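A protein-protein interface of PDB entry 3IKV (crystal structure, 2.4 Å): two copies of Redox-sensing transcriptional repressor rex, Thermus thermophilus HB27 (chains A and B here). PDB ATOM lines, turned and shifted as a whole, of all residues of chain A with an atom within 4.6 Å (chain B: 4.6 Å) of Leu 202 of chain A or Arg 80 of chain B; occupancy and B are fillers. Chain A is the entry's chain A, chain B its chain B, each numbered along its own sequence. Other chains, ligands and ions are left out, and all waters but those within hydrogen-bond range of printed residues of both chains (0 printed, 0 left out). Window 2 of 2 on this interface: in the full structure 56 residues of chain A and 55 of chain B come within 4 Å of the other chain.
Hydrophobic or aromatic side chains of chain B that line the printed part of chain A: Trp 82.
Of the 7 printed residues of chain A, 3 touch a printed residue of chain B.
Printed residues of chain A that touch a printed residue of chain B: Ser 198, Ile 201 and Leu 202.
Hydrophobic or aromatic side chains of chain A that line the printed part of chain B: Ile 201 and Leu 202.
Among the printed residues, 6 pairs touch across the chains.
The backbone NH (N) of Trp 82 of chain B lies within hydrogen-bond range of the backbone carbonyl oxygen (O) of Ser 105 of chain B (2.9 Å).
The backbone carbonyl oxygen of Gly 77 of chain B is in hydrogen-bond range of the indole nitrogen of Trp 82 of chain B, 2.9 Å away.
The side-chain hydroxyl (OG) of Ser 198 of chain A is in hydrogen-bond range of the backbone carbonyl oxygen (O) of Gly 77 of chain B.
OG of Ser 198 of chain A is in hydrogen-bond range of NE1 of Trp 82 of chain B (3.0 Å).
Of the printed residues of chain B, Ile 201 of chain A touches Trp 82 (3.7 Å).
Of chain B, only Gly 77, Arg 80 and Trp 82 come within 4 Å of Leu 202 of chain A.
Printed residues of chain A within 4 Å of Gly 77 of chain B: Ser 198 (3.3 Å) and Leu 202 (3.4 Å).
Of the printed residues of chain A, Trp 82 of chain B touches Ser 198, Ile 201 and Leu 202.
Ser 105 of chain B touches none of the printed residues of chain A.
The nearest printed residue of chain B that does not touch Leu 202 of chain A is Leu 78 of chain B (5.8 Å).
The nearest printed residue of chain A that does not touch Arg 80 of chain B is Ser 198 of chain A (5.8 Å).
The nearest printed residue of chain A that does not touch Trp 82 of chain B is Phe 199 of chain A (5.4 Å).
Trp 82 of chain B touches Ile 201 of chain A (CZ3 to CD1, 3.7 Å).
CA of Gly 77 of chain B touches CD1 of Leu 202 of chain A (3.4 Å).
Leu 202 of chain A touches Arg 80 of chain B (CD1 to NE, 3.7 Å).
CZ2 of Trp 82 of chain B touches CG of Leu 202 of chain A (3.8 Å).
No position is printed for both chains.
Of the 6 pairs that touch across the chains among the printed residues, none has its exchanged pair printed and touching as well.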
ATOM      1  N   SER A 198     -20.791 -14.053 -12.878  1.00  0.00           N
ATOM      2  CA  SER A 198     -20.183 -15.192 -12.201  1.00  0.00           C
ATOM      3  C   SER A 198     -19.066 -15.708 -13.088  1.00  0.00           C
ATOM      4  O   SER A 198     -17.913 -15.802 -12.674  1.00  0.00           O
ATOM      5  CB  SER A 198     -21.216 -16.296 -11.981  1.00  0.00           C
ATOM      6  OG  SER A 198     -20.635 -17.399 -11.306  1.00  0.00           O
ATOM      7  N   PHE A 199     -19.424 -16.030 -14.321  1.00  0.00           N
ATOM      8  CA  PHE A 199     -18.455 -16.531 -15.279  1.00  0.00           C
ATOM      9  C   PHE A 199     -17.272 -15.583 -15.494  1.00  0.00           C
ATOM     10  O   PHE A 199     -16.118 -16.010 -15.499  1.00  0.00           O
ATOM     11  CB  PHE A 199     -19.127 -16.776 -16.612  1.00  0.00           C
ATOM     12  CG  PHE A 199     -18.213 -17.352 -17.611  1.00  0.00           C
ATOM     13  CD1 PHE A 199     -17.878 -18.700 -17.561  1.00  0.00           C
ATOM     14  CD2 PHE A 199     -17.617 -16.540 -18.563  1.00  0.00           C
ATOM     15  CE1 PHE A 199     -16.952 -19.235 -18.444  1.00  0.00           C
ATOM     16  CE2 PHE A 199     -16.692 -17.060 -19.450  1.00  0.00           C
ATOM     17  CZ  PHE A 199     -16.357 -18.413 -19.392  1.00  0.00           C
ATOM     18  N   ALA A 200     -17.566 -14.300 -15.684  1.00  0.00           N
ATOM     19  CA  ALA A 200     -16.522 -13.300 -15.890  1.00  0.00           C
ATOM     20  C   ALA A 200     -15.548 -13.191 -14.703  1.00  0.00           C
ATOM     21  O   ALA A 200     -14.345 -13.042 -14.915  1.00  0.00           O
ATOM     22  CB  ALA A 200     -17.157 -11.937 -16.178  1.00  0.00           C
ATOM     23  N   ILE A 201     -16.055 -13.259 -13.470  1.00  0.00           N
ATOM     24  CA  ILE A 201     -15.195 -13.173 -12.283  1.00  0.00           C
ATOM     25  C   ILE A 201     -14.303 -14.418 -12.187  1.00  0.00           C
ATOM     26  O   ILE A 201     -13.185 -14.352 -11.683  1.00  0.00           O
ATOM     27  CB  ILE A 201     -16.030 -13.021 -10.958  1.00  0.00           C
ATOM     28  CG1 ILE A 201     -16.877 -11.741 -11.004  1.00  0.00           C
ATOM     29  CG2 ILE A 201     -15.094 -12.948  -9.739  1.00  0.00           C
ATOM     30  CD1 ILE A 201     -17.801 -11.558  -9.803  1.00  0.00           C
ATOM     31  N   LEU A 202     -14.786 -15.551 -12.685  1.00  0.00           N
ATOM     32  CA  LEU A 202     -14.006 -16.781 -12.636  1.00  0.00           C
ATOM     33  C   LEU A 202     -13.075 -16.928 -13.832  1.00  0.00           C
ATOM     34  O   LEU A 202     -12.216 -17.803 -13.849  1.00  0.00           O
ATOM     35  CB  LEU A 202     -14.935 -17.995 -12.571  1.00  0.00           C
ATOM     36  CG  LEU A 202     -15.780 -18.103 -11.306  1.00  0.00           C
ATOM     37  CD1 LEU A 202     -16.690 -19.331 -11.402  1.00  0.00           C
ATOM     38  CD2 LEU A 202     -14.868 -18.203 -10.098  1.00  0.00           C
ATOM     39  N   ASN A 203     -13.251 -16.080 -14.835  1.00  0.00           N
ATOM     40  CA  ASN A 203     -12.420 -16.145 -16.029  1.00  0.00           C
ATOM     41  C   ASN A 203     -12.043 -14.745 -16.504  1.00  0.00           C
ATOM     42  O   ASN A 203     -12.516 -14.271 -17.536  1.00  0.00           O
ATOM     43  CB  ASN A 203     -13.155 -16.900 -17.141  1.00  0.00           C
ATOM     44  CG  ASN A 203     -13.481 -18.337 -16.754  1.00  0.00           C
ATOM     45  OD1 ASN A 203     -14.369 -18.591 -15.934  1.00  0.00           O
ATOM     46  ND2 ASN A 203     -12.752 -19.285 -17.339  1.00  0.00           N
ATOM     47  N   PRO A 204     -11.177 -14.062 -15.744  1.00  0.00           N
ATOM     48  CA  PRO A 204     -10.741 -12.707 -16.091  1.00  0.00           C
ATOM     49  C   PRO A 204     -10.027 -12.575 -17.438  1.00  0.00           C
ATOM     50  O   PRO A 204     -10.486 -11.844 -18.308  1.00  0.00           O
ATOM     51  CB  PRO A 204      -9.869 -12.306 -14.900  1.00  0.00           C
ATOM     52  CG  PRO A 204      -9.364 -13.609 -14.377  1.00  0.00           C
ATOM     53  CD  PRO A 204     -10.564 -14.511 -14.484  1.00  0.00           C
ATOM     54  N   GLY B  77     -19.981 -21.210 -12.941  1.00  0.00           N
ATOM     55  CA  GLY B  77     -19.720 -20.874 -11.555  1.00  0.00           C
ATOM     56  C   GLY B  77     -20.964 -20.838 -10.695  1.00  0.00           C
ATOM     57  O   GLY B  77     -20.974 -20.206  -9.634  1.00  0.00           O
ATOM     58  N   LEU B  78     -22.023 -21.506 -11.140  1.00  0.00           N
ATOM     59  CA  LEU B  78     -23.265 -21.529 -10.374  1.00  0.00           C
ATOM     60  C   LEU B  78     -23.225 -22.521  -9.215  1.00  0.00           C
ATOM     61  O   LEU B  78     -24.099 -22.504  -8.349  1.00  0.00           O
ATOM     62  CB  LEU B  78     -24.453 -21.849 -11.286  1.00  0.00           C
ATOM     63  CG  LEU B  78     -24.958 -20.734 -12.206  1.00  0.00           C
ATOM     64  CD1 LEU B  78     -26.068 -21.311 -13.075  1.00  0.00           C
ATOM     65  CD2 LEU B  78     -25.482 -19.538 -11.392  1.00  0.00           C
ATOM     66  N   ASN B  79     -22.221 -23.392  -9.205  1.00  0.00           N
ATOM     67  CA  ASN B  79     -22.083 -24.364  -8.129  1.00  0.00           C
ATOM     68  C   ASN B  79     -21.268 -23.769  -6.965  1.00  0.00           C
ATOM     69  O   ASN B  79     -20.693 -24.487  -6.151  1.00  0.00           O
ATOM     70  CB  ASN B  79     -21.435 -25.659  -8.632  1.00  0.00           C
ATOM     71  CG  ASN B  79     -20.030 -25.448  -9.153  1.00  0.00           C
ATOM     72  OD1 ASN B  79     -19.420 -24.399  -8.930  1.00  0.00           O
ATOM     73  ND2 ASN B  79     -19.501 -26.452  -9.846  1.00  0.00           N
ATOM     74  N   ARG B  80     -21.221 -22.446  -6.899  1.00  0.00           N
ATOM     75  CA  ARG B  80     -20.537 -21.757  -5.808  1.00  0.00           C
ATOM     76  C   ARG B  80     -21.611 -20.891  -5.172  1.00  0.00           C
ATOM     77  O   ARG B  80     -22.715 -20.800  -5.697  1.00  0.00           O
ATOM     78  CB  ARG B  80     -19.420 -20.858  -6.337  1.00  0.00           C
ATOM     79  CG  ARG B  80     -18.255 -21.606  -6.943  1.00  0.00           C
ATOM     80  CD  ARG B  80     -17.406 -20.665  -7.768  1.00  0.00           C
ATOM     81  NE  ARG B  80     -16.239 -21.327  -8.338  1.00  0.00           N
ATOM     82  CZ  ARG B  80     -15.108 -21.553  -7.679  1.00  0.00           C
ATOM     83  NH1 ARG B  80     -14.977 -21.173  -6.417  1.00  0.00           N
ATOM     84  NH2 ARG B  80     -14.096 -22.157  -8.288  1.00  0.00           N
ATOM     85  N   LYS B  81     -21.317 -20.284  -4.033  1.00  0.00           N
ATOM     86  CA  LYS B  81     -22.287 -19.390  -3.409  1.00  0.00           C
ATOM     87  C   LYS B  81     -21.681 -17.996  -3.452  1.00  0.00           C
ATOM     88  O   LYS B  81     -20.673 -17.724  -2.792  1.00  0.00           O
ATOM     89  CB  LYS B  81     -22.582 -19.770  -1.959  1.00  0.00           C
ATOM     90  CG  LYS B  81     -23.482 -18.739  -1.277  1.00  0.00           C
ATOM     91  CD  LYS B  81     -23.736 -19.038   0.193  1.00  0.00           C
ATOM     92  CE  LYS B  81     -24.535 -20.321   0.366  1.00  0.00           C
ATOM     93  NZ  LYS B  81     -25.849 -20.265  -0.336  1.00  0.00           N
ATOM     94  N   TRP B  82     -22.286 -17.123  -4.245  1.00  0.00           N
ATOM     95  CA  TRP B  82     -21.792 -15.762  -4.382  1.00  0.00           C
ATOM     96  C   TRP B  82     -22.501 -14.788  -3.462  1.00  0.00           C
ATOM     97  O   TRP B  82     -23.729 -14.838  -3.313  1.00  0.00           O
ATOM     98  CB  TRP B  82     -21.966 -15.275  -5.816  1.00  0.00           C
ATOM     99  CG  TRP B  82     -21.201 -16.052  -6.810  1.00  0.00           C
ATOM    100  CD1 TRP B  82     -21.590 -17.203  -7.424  1.00  0.00           C
ATOM    101  CD2 TRP B  82     -19.919 -15.717  -7.351  1.00  0.00           C
ATOM    102  NE1 TRP B  82     -20.633 -17.605  -8.321  1.00  0.00           N
ATOM    103  CE2 TRP B  82     -19.596 -16.710  -8.296  1.00  0.00           C
ATOM    104  CE3 TRP B  82     -19.013 -14.673  -7.125  1.00  0.00           C
ATOM    105  CZ2 TRP B  82     -18.404 -16.689  -9.027  1.00  0.00           C
ATOM    106  CZ3 TRP B  82     -17.830 -14.650  -7.852  1.00  0.00           C
ATOM    107  CH2 TRP B  82     -17.536 -15.657  -8.794  1.00  0.00           C
ATOM    108  N   SER B 105     -27.445 -20.071  -5.620  1.00  0.00           N
ATOM    109  CA  SER B 105     -26.163 -19.546  -6.076  1.00  0.00           C
ATOM    110  C   SER B 105     -25.862 -18.090  -5.710  1.00  0.00           C
ATOM    111  O   SER B 105     -24.696 -17.684  -5.669  1.00  0.00           O
ATOM    112  CB  SER B 105     -26.057 -19.684  -7.594  1.00  0.00           C
ATOM    113  OG  SER B 105     -26.036 -21.043  -7.985  1.00  0.00           O
